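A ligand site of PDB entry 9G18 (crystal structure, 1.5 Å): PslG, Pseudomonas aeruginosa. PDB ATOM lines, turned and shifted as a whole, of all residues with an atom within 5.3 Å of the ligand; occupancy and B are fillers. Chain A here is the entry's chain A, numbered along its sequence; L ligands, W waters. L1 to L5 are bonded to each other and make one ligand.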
ATOM      1  N   GLN A  26     -10.222 -36.520  27.167  1.00  0.00           N
ATOM      2  CA  GLN A  26      -8.775 -36.598  26.934  1.00  0.00           C
ATOM      3  C   GLN A  26      -8.332 -38.054  27.146  1.00  0.00           C
ATOM      4  O   GLN A  26      -7.393 -38.355  27.899  1.00  0.00           O
ATOM      5  CB  GLN A  26      -8.078 -35.652  27.918  1.00  0.00           C
ATOM      6  CG  GLN A  26      -7.978 -34.203  27.413  1.00  0.00           C
ATOM      7  CD  GLN A  26      -9.317 -33.519  27.269  1.00  0.00           C
ATOM      8  OE1 GLN A  26     -10.139 -33.470  28.177  1.00  0.00           O
ATOM      9  NE2 GLN A  26      -9.598 -33.058  26.040  1.00  0.00           N
ATOM     10  N   TRP A  29      -4.825 -39.571  27.431  1.00  0.00           N
ATOM     11  CA  TRP A  29      -3.996 -39.305  28.598  1.00  0.00           C
ATOM     12  C   TRP A  29      -4.089 -40.424  29.614  1.00  0.00           C
ATOM     13  O   TRP A  29      -3.452 -40.327  30.669  1.00  0.00           O
ATOM     14  CB  TRP A  29      -4.466 -38.030  29.320  1.00  0.00           C
ATOM     15  CG  TRP A  29      -4.267 -36.752  28.545  1.00  0.00           C
ATOM     16  CD1 TRP A  29      -4.562 -36.482  27.237  1.00  0.00           C
ATOM     17  CD2 TRP A  29      -3.756 -35.522  29.116  1.00  0.00           C
ATOM     18  NE1 TRP A  29      -4.316 -35.147  26.973  1.00  0.00           N
ATOM     19  CE2 TRP A  29      -3.797 -34.548  28.108  1.00  0.00           C
ATOM     20  CE3 TRP A  29      -3.289 -35.177  30.400  1.00  0.00           C
ATOM     21  CZ2 TRP A  29      -3.381 -33.236  28.345  1.00  0.00           C
ATOM     22  CZ3 TRP A  29      -2.835 -33.887  30.635  1.00  0.00           C
ATOM     23  CH2 TRP A  29      -2.905 -32.932  29.613  1.00  0.00           C
ATOM     24  N   ASP A  53      -9.086 -34.536  21.399  1.00  0.00           N
ATOM     25  CA  ASP A  53      -7.990 -33.793  20.764  1.00  0.00           C
ATOM     26  C   ASP A  53      -6.897 -34.726  20.263  1.00  0.00           C
ATOM     27  O   ASP A  53      -6.439 -35.616  20.981  1.00  0.00           O
ATOM     28  CB  ASP A  53      -7.390 -32.802  21.773  1.00  0.00           C
ATOM     29  CG  ASP A  53      -6.891 -33.415  23.071  1.00  0.00           C
ATOM     30  OD1 ASP A  53      -7.649 -34.214  23.724  1.00  0.00           O
ATOM     31  OD2 ASP A  53      -5.726 -33.179  23.449  1.00  0.00           O
ATOM     32  N   HIS A  55      -2.941 -34.332  18.436  1.00  0.00           N
ATOM     33  CA  HIS A  55      -1.846 -33.408  18.192  1.00  0.00           C
ATOM     34  C   HIS A  55      -0.943 -34.052  17.153  1.00  0.00           C
ATOM     35  O   HIS A  55      -0.364 -35.097  17.446  1.00  0.00           O
ATOM     36  CB  HIS A  55      -1.075 -33.106  19.487  1.00  0.00           C
ATOM     37  CG  HIS A  55      -2.075 -32.583  20.485  1.00  0.00           C
ATOM     38  ND1 HIS A  55      -2.363 -31.228  20.615  1.00  0.00           N
ATOM     39  CD2 HIS A  55      -2.934 -33.246  21.303  1.00  0.00           C
ATOM     40  CE1 HIS A  55      -3.344 -31.077  21.490  1.00  0.00           C
ATOM     41  NE2 HIS A  55      -3.723 -32.286  21.913  1.00  0.00           N
ATOM     42  N   ASP A  57       2.015 -33.560  16.097  1.00  0.00           N
ATOM     43  CA  ASP A  57       3.419 -33.817  16.423  1.00  0.00           C
ATOM     44  C   ASP A  57       3.569 -34.990  17.398  1.00  0.00           C
ATOM     45  O   ASP A  57       4.700 -35.436  17.656  1.00  0.00           O
ATOM     46  CB  ASP A  57       4.185 -32.585  16.901  1.00  0.00           C
ATOM     47  CG  ASP A  57       3.891 -32.131  18.324  1.00  0.00           C
ATOM     48  OD1 ASP A  57       2.948 -32.670  18.952  1.00  0.00           O
ATOM     49  OD2 ASP A  57       4.648 -31.253  18.798  1.00  0.00           O
ATOM     50  N   ARG A  58       2.460 -35.497  17.945  1.00  0.00           N
ATOM     51  CA  ARG A  58       2.488 -36.709  18.773  1.00  0.00           C
ATOM     52  C   ARG A  58       2.155 -37.952  17.939  1.00  0.00           C
ATOM     53  O   ARG A  58       2.588 -39.057  18.298  1.00  0.00           O
ATOM     54  CB  ARG A  58       1.400 -36.579  19.875  1.00  0.00           C
ATOM     55  CG  ARG A  58       1.759 -35.415  20.802  1.00  0.00           C
ATOM     56  CD  ARG A  58       0.762 -35.322  21.976  1.00  0.00           C
ATOM     57  NE  ARG A  58       1.005 -34.043  22.665  1.00  0.00           N
ATOM     58  CZ  ARG A  58       0.591 -33.837  23.910  1.00  0.00           C
ATOM     59  NH1 ARG A  58      -0.194 -34.747  24.525  1.00  0.00           N
ATOM     60  NH2 ARG A  58       0.993 -32.739  24.531  1.00  0.00           N
ATOM     61  N   TYR A  88     -10.507 -33.775  16.604  1.00  0.00           N
ATOM     62  CA  TYR A  88      -9.859 -32.694  15.844  1.00  0.00           C
ATOM     63  C   TYR A  88      -8.349 -32.939  15.824  1.00  0.00           C
ATOM     64  O   TYR A  88      -7.812 -33.519  16.775  1.00  0.00           O
ATOM     65  CB  TYR A  88     -10.167 -31.334  16.471  1.00  0.00           C
ATOM     66  CG  TYR A  88      -9.590 -30.985  17.848  1.00  0.00           C
ATOM     67  CD1 TYR A  88     -10.340 -31.239  19.016  1.00  0.00           C
ATOM     68  CD2 TYR A  88      -8.356 -30.307  18.009  1.00  0.00           C
ATOM     69  CE1 TYR A  88      -9.926 -30.826  20.269  1.00  0.00           C
ATOM     70  CE2 TYR A  88      -7.918 -29.914  19.274  1.00  0.00           C
ATOM     71  CZ  TYR A  88      -8.731 -30.133  20.386  1.00  0.00           C
ATOM     72  OH  TYR A  88      -8.318 -29.677  21.606  1.00  0.00           O
ATOM     73  N   VAL A  90      -4.722 -30.970  15.483  1.00  0.00           N
ATOM     74  CA  VAL A  90      -4.166 -29.623  15.560  1.00  0.00           C
ATOM     75  C   VAL A  90      -2.645 -29.705  15.678  1.00  0.00           C
ATOM     76  O   VAL A  90      -2.093 -30.707  16.192  1.00  0.00           O
ATOM     77  CB  VAL A  90      -4.766 -28.832  16.746  1.00  0.00           C
ATOM     78  CG1 VAL A  90      -4.375 -29.452  18.106  1.00  0.00           C
ATOM     79  CG2 VAL A  90      -4.360 -27.328  16.738  1.00  0.00           C
ATOM     80  N   GLY A  91      -2.021 -28.587  15.306  1.00  0.00           N
ATOM     81  CA  GLY A  91      -0.568 -28.440  15.454  1.00  0.00           C
ATOM     82  C   GLY A  91       0.170 -29.005  14.244  1.00  0.00           C
ATOM     83  O   GLY A  91      -0.355 -29.839  13.517  1.00  0.00           O
ATOM     84  N   PHE A 105       7.857 -23.198  20.624  1.00  0.00           N
ATOM     85  CA  PHE A 105       6.488 -23.648  20.420  1.00  0.00           C
ATOM     86  C   PHE A 105       6.349 -24.231  19.004  1.00  0.00           C
ATOM     87  O   PHE A 105       5.594 -23.726  18.173  1.00  0.00           O
ATOM     88  CB  PHE A 105       5.483 -22.499  20.604  1.00  0.00           C
ATOM     89  CG  PHE A 105       5.687 -21.783  21.936  1.00  0.00           C
ATOM     90  CD1 PHE A 105       5.371 -22.421  23.143  1.00  0.00           C
ATOM     91  CD2 PHE A 105       6.197 -20.488  21.980  1.00  0.00           C
ATOM     92  CE1 PHE A 105       5.546 -21.781  24.357  1.00  0.00           C
ATOM     93  CE2 PHE A 105       6.381 -19.843  23.205  1.00  0.00           C
ATOM     94  CZ  PHE A 105       6.064 -20.487  24.395  1.00  0.00           C
ATOM     95  N   ASP A 107       5.035 -26.674  17.436  1.00  0.00           N
ATOM     96  CA  ASP A 107       3.795 -27.179  16.828  1.00  0.00           C
ATOM     97  C   ASP A 107       2.703 -26.105  16.801  1.00  0.00           C
ATOM     98  O   ASP A 107       1.645 -26.385  16.231  1.00  0.00           O
ATOM     99  CB  ASP A 107       3.276 -28.469  17.459  1.00  0.00           C
ATOM    100  CG  ASP A 107       2.216 -28.319  18.576  1.00  0.00           C
ATOM    101  OD1 ASP A 107       2.351 -27.358  19.356  1.00  0.00           O
ATOM    102  OD2 ASP A 107       1.318 -29.212  18.722  1.00  0.00           O
ATOM    103  N   GLN A 108       2.939 -24.904  17.352  1.00  0.00           N
ATOM    104  CA  GLN A 108       1.894 -23.884  17.425  1.00  0.00           C
ATOM    105  C   GLN A 108       1.885 -22.985  16.188  1.00  0.00           C
ATOM    106  O   GLN A 108       1.249 -21.943  16.160  1.00  0.00           O
ATOM    107  CB  GLN A 108       2.053 -23.078  18.718  1.00  0.00           C
ATOM    108  CG  GLN A 108       1.783 -23.948  19.927  1.00  0.00           C
ATOM    109  CD  GLN A 108       1.931 -23.246  21.258  1.00  0.00           C
ATOM    110  OE1 GLN A 108       2.172 -22.030  21.337  1.00  0.00           O
ATOM    111  NE2 GLN A 108       1.724 -24.019  22.323  1.00  0.00           N
ATOM    112  N   ASN A 138      -7.688 -26.081  15.683  1.00  0.00           N
ATOM    113  CA  ASN A 138      -8.379 -25.627  16.891  1.00  0.00           C
ATOM    114  C   ASN A 138      -7.988 -24.160  17.107  1.00  0.00           C
ATOM    115  O   ASN A 138      -6.811 -23.817  16.986  1.00  0.00           O
ATOM    116  CB  ASN A 138      -7.961 -26.500  18.085  1.00  0.00           C
ATOM    117  CG  ASN A 138      -8.712 -26.186  19.355  1.00  0.00           C
ATOM    118  OD1 ASN A 138      -9.932 -26.363  19.361  1.00  0.00           O
ATOM    119  ND2 ASN A 138      -8.047 -25.832  20.470  1.00  0.00           N
ATOM    120  N   GLU A 139      -8.993 -23.328  17.488  1.00  0.00           N
ATOM    121  CA  GLU A 139      -8.812 -21.933  17.878  1.00  0.00           C
ATOM    122  C   GLU A 139      -7.733 -21.230  17.062  1.00  0.00           C
ATOM    123  O   GLU A 139      -6.791 -20.656  17.638  1.00  0.00           O
ATOM    124  CB  GLU A 139      -8.475 -21.870  19.378  1.00  0.00           C
ATOM    125  CG  GLU A 139      -9.640 -22.424  20.224  1.00  0.00           C
ATOM    126  CD  GLU A 139      -9.574 -22.117  21.695  1.00  0.00           C
ATOM    127  OE1 GLU A 139      -8.539 -21.585  22.165  1.00  0.00           O
ATOM    128  OE2 GLU A 139     -10.611 -22.317  22.379  1.00  0.00           O
ATOM    129  N   GLY A 144      -1.765 -18.954  20.655  1.00  0.00           N
ATOM    130  CA  GLY A 144      -1.223 -20.224  21.129  1.00  0.00           C
ATOM    131  C   GLY A 144      -1.538 -21.411  20.237  1.00  0.00           C
ATOM    132  O   GLY A 144      -0.988 -22.478  20.485  1.00  0.00           O
ATOM    133  N   PHE A 145      -2.444 -21.275  19.261  1.00  0.00           N
ATOM    134  CA  PHE A 145      -2.663 -22.350  18.289  1.00  0.00           C
ATOM    135  C   PHE A 145      -2.211 -21.995  16.862  1.00  0.00           C
ATOM    136  O   PHE A 145      -2.239 -22.860  15.970  1.00  0.00           O
ATOM    137  CB  PHE A 145      -4.132 -22.824  18.275  1.00  0.00           C
ATOM    138  CG  PHE A 145      -4.482 -23.520  19.566  1.00  0.00           C
ATOM    139  CD1 PHE A 145      -4.179 -24.883  19.752  1.00  0.00           C
ATOM    140  CD2 PHE A 145      -5.177 -22.830  20.564  1.00  0.00           C
ATOM    141  CE1 PHE A 145      -4.531 -25.518  20.948  1.00  0.00           C
ATOM    142  CE2 PHE A 145      -5.509 -23.474  21.767  1.00  0.00           C
ATOM    143  CZ  PHE A 145      -5.195 -24.822  21.964  1.00  0.00           C
ATOM    144  N   HIS A 211     -16.151 -21.378  21.002  1.00  0.00           N
ATOM    145  CA  HIS A 211     -15.809 -21.778  22.369  1.00  0.00           C
ATOM    146  C   HIS A 211     -16.054 -20.581  23.269  1.00  0.00           C
ATOM    147  O   HIS A 211     -15.124 -19.887  23.705  1.00  0.00           O
ATOM    148  CB  HIS A 211     -14.338 -22.187  22.509  1.00  0.00           C
ATOM    149  CG  HIS A 211     -14.041 -23.425  21.699  1.00  0.00           C
ATOM    150  ND1 HIS A 211     -12.727 -23.854  21.547  1.00  0.00           N
ATOM    151  CD2 HIS A 211     -14.819 -24.333  21.010  1.00  0.00           C
ATOM    152  CE1 HIS A 211     -12.712 -25.017  20.854  1.00  0.00           C
ATOM    153  NE2 HIS A 211     -13.967 -25.326  20.485  1.00  0.00           N
ATOM    154  N   TYR A 213     -16.191 -19.221  26.171  1.00  0.00           N
ATOM    155  CA  TYR A 213     -15.869 -19.142  27.593  1.00  0.00           C
ATOM    156  C   TYR A 213     -16.030 -17.697  28.066  1.00  0.00           C
ATOM    157  O   TYR A 213     -15.583 -16.758  27.374  1.00  0.00           O
ATOM    158  CB  TYR A 213     -14.386 -19.508  27.759  1.00  0.00           C
ATOM    159  CG  TYR A 213     -14.062 -20.987  27.572  1.00  0.00           C
ATOM    160  CD1 TYR A 213     -14.110 -21.862  28.670  1.00  0.00           C
ATOM    161  CD2 TYR A 213     -13.597 -21.480  26.325  1.00  0.00           C
ATOM    162  CE1 TYR A 213     -13.739 -23.211  28.543  1.00  0.00           C
ATOM    163  CE2 TYR A 213     -13.210 -22.823  26.200  1.00  0.00           C
ATOM    164  CZ  TYR A 213     -13.214 -23.655  27.328  1.00  0.00           C
ATOM    165  OH  TYR A 213     -12.815 -24.962  27.215  1.00  0.00           O
ATOM    166  N   GLU A 250     -16.569 -26.265  22.941  1.00  0.00           N
ATOM    167  CA  GLU A 250     -16.043 -26.152  24.289  1.00  0.00           C
ATOM    168  C   GLU A 250     -16.698 -24.971  25.006  1.00  0.00           C
ATOM    169  O   GLU A 250     -17.036 -23.954  24.398  1.00  0.00           O
ATOM    170  CB  GLU A 250     -14.524 -25.843  24.412  1.00  0.00           C
ATOM    171  CG  GLU A 250     -13.635 -26.912  23.769  1.00  0.00           C
ATOM    172  CD  GLU A 250     -12.170 -26.626  24.027  1.00  0.00           C
ATOM    173  OE1 GLU A 250     -11.809 -25.856  24.963  1.00  0.00           O
ATOM    174  OE2 GLU A 250     -11.335 -27.239  23.253  1.00  0.00           O
ATOM    175  N   PHE A 293     -16.525 -28.682  28.454  1.00  0.00           N
ATOM    176  CA  PHE A 293     -15.109 -28.928  28.689  1.00  0.00           C
ATOM    177  C   PHE A 293     -14.971 -29.101  30.205  1.00  0.00           C
ATOM    178  O   PHE A 293     -15.166 -28.128  30.920  1.00  0.00           O
ATOM    179  CB  PHE A 293     -14.268 -27.767  28.122  1.00  0.00           C
ATOM    180  CG  PHE A 293     -12.793 -28.122  28.143  1.00  0.00           C
ATOM    181  CD1 PHE A 293     -12.237 -28.811  27.067  1.00  0.00           C
ATOM    182  CD2 PHE A 293     -11.989 -27.820  29.251  1.00  0.00           C
ATOM    183  CE1 PHE A 293     -10.881 -29.191  27.078  1.00  0.00           C
ATOM    184  CE2 PHE A 293     -10.649 -28.225  29.291  1.00  0.00           C
ATOM    185  CZ  PHE A 293     -10.087 -28.920  28.192  1.00  0.00           C
ATOM    186  N   LEU A 298      -7.277 -33.564  34.881  1.00  0.00           N
ATOM    187  CA  LEU A 298      -6.061 -34.019  34.206  1.00  0.00           C
ATOM    188  C   LEU A 298      -4.882 -33.923  35.173  1.00  0.00           C
ATOM    189  O   LEU A 298      -4.922 -33.179  36.144  1.00  0.00           O
ATOM    190  CB  LEU A 298      -5.849 -33.124  32.975  1.00  0.00           C
ATOM    191  CG  LEU A 298      -6.944 -33.195  31.906  1.00  0.00           C
ATOM    192  CD1 LEU A 298      -6.727 -32.108  30.835  1.00  0.00           C
ATOM    193  CD2 LEU A 298      -7.025 -34.613  31.300  1.00  0.00           C
ATOM    194  N   ARG A 301       0.616 -32.884  33.476  1.00  0.00           N
ATOM    195  CA  ARG A 301       0.923 -32.541  32.098  1.00  0.00           C
ATOM    196  C   ARG A 301       0.108 -31.338  31.624  1.00  0.00           C
ATOM    197  O   ARG A 301       0.512 -30.642  30.690  1.00  0.00           O
ATOM    198  CB  ARG A 301       0.732 -33.694  31.102  1.00  0.00           C
ATOM    199  CG  ARG A 301       1.712 -34.833  31.366  1.00  0.00           C
ATOM    200  CD  ARG A 301       1.342 -36.048  30.549  1.00  0.00           C
ATOM    201  NE  ARG A 301       0.167 -36.689  31.181  1.00  0.00           N
ATOM    202  CZ  ARG A 301      -0.442 -37.801  30.719  1.00  0.00           C
ATOM    203  NH1 ARG A 301      -0.079 -38.307  29.554  1.00  0.00           N
ATOM    204  NH2 ARG A 301      -1.426 -38.371  31.424  1.00  0.00           N
ATOM    205  N   ARG A 305      -4.625 -24.435  35.572  1.00  0.00           N
ATOM    206  CA  ARG A 305      -6.057 -24.210  35.426  1.00  0.00           C
ATOM    207  C   ARG A 305      -6.687 -25.400  34.694  1.00  0.00           C
ATOM    208  O   ARG A 305      -7.793 -25.860  35.034  1.00  0.00           O
ATOM    209  CB  ARG A 305      -6.310 -22.933  34.615  1.00  0.00           C
ATOM    210  CG  ARG A 305      -7.798 -22.730  34.304  1.00  0.00           C
ATOM    211  CD  ARG A 305      -8.059 -21.269  33.921  1.00  0.00           C
ATOM    212  NE  ARG A 305      -7.061 -20.757  32.983  1.00  0.00           N
ATOM    213  CZ  ARG A 305      -7.124 -20.904  31.670  1.00  0.00           C
ATOM    214  NH1 ARG A 305      -8.085 -21.607  31.111  1.00  0.00           N
ATOM    215  NH2 ARG A 305      -6.228 -20.307  30.927  1.00  0.00           N
ATOM    216  N   ASP A 306      -5.965 -25.959  33.703  1.00  0.00           N
ATOM    217  CA  ASP A 306      -6.595 -26.945  32.825  1.00  0.00           C
ATOM    218  C   ASP A 306      -6.793 -28.297  33.515  1.00  0.00           C
ATOM    219  O   ASP A 306      -7.485 -29.158  32.949  1.00  0.00           O
ATOM    220  CB  ASP A 306      -5.822 -27.145  31.514  1.00  0.00           C
ATOM    221  CG  ASP A 306      -5.961 -26.011  30.508  1.00  0.00           C
ATOM    222  OD1 ASP A 306      -6.604 -25.019  30.848  1.00  0.00           O
ATOM    223  OD2 ASP A 306      -5.431 -26.150  29.358  1.00  0.00           O
ATOM    224  N   TYR A 309     -11.034 -28.902  35.100  1.00  0.00           N
ATOM    225  CA  TYR A 309     -12.296 -28.685  34.382  1.00  0.00           C
ATOM    226  C   TYR A 309     -13.209 -29.912  34.426  1.00  0.00           C
ATOM    227  O   TYR A 309     -14.301 -29.852  33.845  1.00  0.00           O
ATOM    228  CB  TYR A 309     -12.048 -28.346  32.894  1.00  0.00           C
ATOM    229  CG  TYR A 309     -11.661 -26.893  32.630  1.00  0.00           C
ATOM    230  CD1 TYR A 309     -12.626 -25.917  32.391  1.00  0.00           C
ATOM    231  CD2 TYR A 309     -10.299 -26.527  32.532  1.00  0.00           C
ATOM    232  CE1 TYR A 309     -12.268 -24.608  32.058  1.00  0.00           C
ATOM    233  CE2 TYR A 309      -9.934 -25.216  32.222  1.00  0.00           C
ATOM    234  CZ  TYR A 309     -10.920 -24.262  32.005  1.00  0.00           C
ATOM    235  OH  TYR A 309     -10.536 -22.984  31.673  1.00  0.00           O
HETATM  236  C1  LIG L   1      -9.412 -24.057  24.959  1.00  0.00           C
HETATM  237  C2  LIG L   1      -8.421 -25.084  24.365  1.00  0.00           C
HETATM  238  O1  LIG L   1      -9.003 -25.649  23.175  1.00  0.00           O
HETATM  239  C3  LIG L   1      -8.023 -26.198  25.357  1.00  0.00           C
HETATM  240  O2  LIG L   1      -6.787 -26.790  24.950  1.00  0.00           O
HETATM  241  C4  LIG L   1      -7.802 -25.685  26.778  1.00  0.00           C
HETATM  242  O3  LIG L   1      -7.565 -26.773  27.666  1.00  0.00           O
HETATM  243  C5  LIG L   1      -9.047 -24.906  27.225  1.00  0.00           C
HETATM  244  N1  LIG L   1      -9.085 -23.702  26.357  1.00  0.00           N
HETATM  245  C6  LIG L   1      -9.060 -24.498  28.692  1.00  0.00           C
HETATM  246  O4  LIG L   1      -7.861 -23.712  28.972  1.00  0.00           O
HETATM  247  C1  LG2 L   2      -6.876 -27.983  24.173  1.00  0.00           C
HETATM  248  C2  LG2 L   2      -5.590 -28.291  23.478  1.00  0.00           C
HETATM  249  C3  LG2 L   2      -4.550 -28.704  24.513  1.00  0.00           C
HETATM  250  C4  LG2 L   2      -5.110 -29.883  25.256  1.00  0.00           C
HETATM  251  C5  LG2 L   2      -6.445 -29.568  25.942  1.00  0.00           C
HETATM  252  C6  LG2 L   2      -7.099 -30.872  26.351  1.00  0.00           C
HETATM  253  O1  LG2 L   2      -5.797 -29.392  22.581  1.00  0.00           O
HETATM  254  O2  LG2 L   2      -3.397 -29.150  23.798  1.00  0.00           O
HETATM  255  O3  LG2 L   2      -4.180 -30.247  26.242  1.00  0.00           O
HETATM  256  O4  LG2 L   2      -7.351 -29.056  24.945  1.00  0.00           O
HETATM  257  C1  LG3 L   3      -2.427 -28.183  23.428  1.00  0.00           C
HETATM  258  C2  LG3 L   3      -1.085 -28.602  24.007  1.00  0.00           C
HETATM  259  C3  LG3 L   3      -0.023 -27.678  23.459  1.00  0.00           C
HETATM  260  C4  LG3 L   3      -0.012 -27.717  21.955  1.00  0.00           C
HETATM  261  C5  LG3 L   3      -1.387 -27.381  21.359  1.00  0.00           C
HETATM  262  C6  LG3 L   3      -1.468 -27.619  19.853  1.00  0.00           C
HETATM  263  O1  LG3 L   3      -0.794 -29.956  23.644  1.00  0.00           O
HETATM  264  O2  LG3 L   3       1.273 -28.156  23.916  1.00  0.00           O
HETATM  265  O3  LG3 L   3       0.943 -26.733  21.463  1.00  0.00           O
HETATM  266  O4  LG3 L   3      -2.378 -28.262  21.983  1.00  0.00           O
HETATM  267  O5  LG3 L   3      -1.139 -29.018  19.533  1.00  0.00           O
HETATM  268  C1  LG4 L   4       1.617 -27.634  25.205  1.00  0.00           C
HETATM  269  C2  LG4 L   4       2.525 -28.603  25.901  1.00  0.00           C
HETATM  270  C3  LG4 L   4       2.943 -28.010  27.208  1.00  0.00           C
HETATM  271  C4  LG4 L   4       3.550 -26.656  27.013  1.00  0.00           C
HETATM  272  C5  LG4 L   4       2.580 -25.748  26.221  1.00  0.00           C
HETATM  273  C6  LG4 L   4       3.166 -24.394  25.899  1.00  0.00           C
HETATM  274  O1  LG4 L   4       3.678 -28.842  25.071  1.00  0.00           O
HETATM  275  O2  LG4 L   4       3.859 -28.886  27.834  1.00  0.00           O
HETATM  276  O3  LG4 L   4       3.757 -26.027  28.309  1.00  0.00           O
HETATM  277  O4  LG4 L   4       2.278 -26.393  24.971  1.00  0.00           O
HETATM  278  O5  LG4 L   4       2.152 -23.570  25.331  1.00  0.00           O
HETATM  279  C1  LG5 L   5       4.034 -30.245  24.811  1.00  0.00           C
HETATM  280  C2  LG5 L   5       5.497 -30.304  24.417  1.00  0.00           C
HETATM  281  C3  LG5 L   5       5.721 -29.684  23.035  1.00  0.00           C
HETATM  282  C4  LG5 L   5       4.771 -30.304  22.022  1.00  0.00           C
HETATM  283  C5  LG5 L   5       3.315 -30.100  22.506  1.00  0.00           C
HETATM  284  C6  LG5 L   5       2.262 -30.758  21.621  1.00  0.00           C
HETATM  285  O1  LG5 L   5       5.906 -31.689  24.452  1.00  0.00           O
HETATM  286  O2  LG5 L   5       7.089 -29.903  22.620  1.00  0.00           O
HETATM  287  O3  LG5 L   5       4.908 -29.647  20.753  1.00  0.00           O
HETATM  288  O4  LG5 L   5       3.193 -30.779  23.794  1.00  0.00           O
HETATM  289  O5  LG5 L   5       2.591 -32.194  21.467  1.00  0.00           O
HETATM  290  O   HOH W   1       6.648 -28.535  27.643  1.00  0.00           O
HETATM  291  O   HOH W   2       2.797 -21.022  26.275  1.00  0.00           O
HETATM  292  O   HOH W   3      -4.684 -24.130  27.866  1.00  0.00           O
HETATM  293  O   HOH W   4     -10.411 -21.562  27.636  1.00  0.00           O
HETATM  294  O   HOH W   5       2.934 -30.931  29.266  1.00  0.00           O
HETATM  295  O   HOH W   6      -2.229 -31.949  25.106  1.00  0.00           O
HETATM  296  O   HOH W   7       7.934 -29.223  20.206  1.00  0.00           O
HETATM  297  O   HOH W   8      -9.848 -29.702  23.688  1.00  0.00           O
HETATM  298  O   HOH W   9       4.696 -26.946  20.384  1.00  0.00           O
HETATM  299  O   HOH W  10       4.487 -26.108  23.101  1.00  0.00           O
HETATM  300  O   HOH W  11       7.897 -32.699  22.339  1.00  0.00           O
HETATM  301  O   HOH W  12       1.257 -25.948  30.017  1.00  0.00           O
HETATM  302  O   HOH W  13       4.377 -33.678  23.010  1.00  0.00           O
HETATM  303  O   HOH W  14      -6.612 -22.207  25.813  1.00  0.00           O
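An oxygen (O3) of LG5 L5 lies within hydrogen-bond range of the side-chain carboxylate (OD2) of Asp 57 (2.5 Å). OD2 of Asp 107 lies within hydrogen-bond range of O5 of LG3 L3 (2.6 Å). An oxygen (O4) of LIG L1 is in hydrogen-bond range of the side-chain carboxylate (OD1) of Asp 306. An oxygen (O5) of LG5 L5 sits at hydrogen-bond distance from the guanidinium group of Arg 58 (2.7 Å). O1 of LG2 L2 lies within hydrogen-bond range of OH of Tyr 88, 2.7 Å away. O5 of LG3 L3 sits at hydrogen-bond distance from ND1 of His 55 (2.7 Å). OE1 of Glu 250 is in salt-bridge range of N1 of LIG L1. An oxygen (O1) of LIG L1 is in hydrogen-bond range of the side-chain amide nitrogen of Asn 138. The side-chain amide nitrogen of Gln 108 is in hydrogen-bond range of an oxygen (O3) of LG3 L3, at 3.0 Å. NH1 of Arg 305 lies within hydrogen-bond range of O4 of LIG L1, at 3.0 Å.
NH1 of Arg 305 lies within salt-bridge range of OD1 of Asp 306 (3.7 Å). A ring nitrogen (NE2) of His 55 is in hydrogen-bond range of the side-chain carboxylate (OD2) of Asp 53 (2.7 Å). The side-chain hydroxyl (OH) of Tyr 213 is in hydrogen-bond range of the side-chain carboxylate (OE1) of Glu 250, at 2.6 Å. OE1 of Gln 108 sits close to O of Gly 144. The guanidinium group (NH1) of Arg 305 lies within hydrogen-bond range of the side-chain hydroxyl (OH) of Tyr 309. The side-chain carboxylate (OE2) of Glu 139 sits at hydrogen-bond distance from a ring nitrogen (ND1) of His 211 (2.7 Å). The side-chain amide nitrogen of Gln 26 sits at hydrogen-bond distance from the side-chain carboxylate of Asp 53. The backbone carbonyl oxygen (O) of Trp 29 sits at hydrogen-bond distance from the guanidinium group (NH2) of Arg 301 (2.9 Å).
Residues that only touch the ligand: Gln 26, Glu 139, Phe 293, Val 90, Phe 145, Tyr 309, Trp 29, Tyr 213, Asp 53 and Phe 105. Hydrophobic or aromatic side chains that line the ligand: Trp 29, His 55, Tyr 88, Val 90, Phe 105, Phe 145, Phe 293 and Tyr 309. The nearest printed residue that does not touch the ligand is Gly 91 (4.2 Å).
Water W5 lies within hydrogen-bond range of an oxygen (O2) of LG4 L4 (2.7 Å) and the backbone carbonyl oxygen (O) of Arg 301 (2.8 Å). Water W9 bridges OD1 of Asp 107 (2.6 Å) and O3 of LG5 L5 (2.7 Å). Water W13 bridges O5 of LG5 L5 (2.8 Å) and NE of Arg 58 (3.4 Å). Water W6 bridges an oxygen (O3) of LG2 L2 and the guanidinium group of Arg 58. Water W8 lies within hydrogen-bond range of OH of Tyr 88 (2.6 Å), O4 of LG2 L2 (2.9 Å) and OE2 of Glu 250 (2.9 Å). Water W3 lies within hydrogen-bond range of OD2 of Asp 306 (2.6 Å) and O4 of LIG L1 (3.4 Å).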
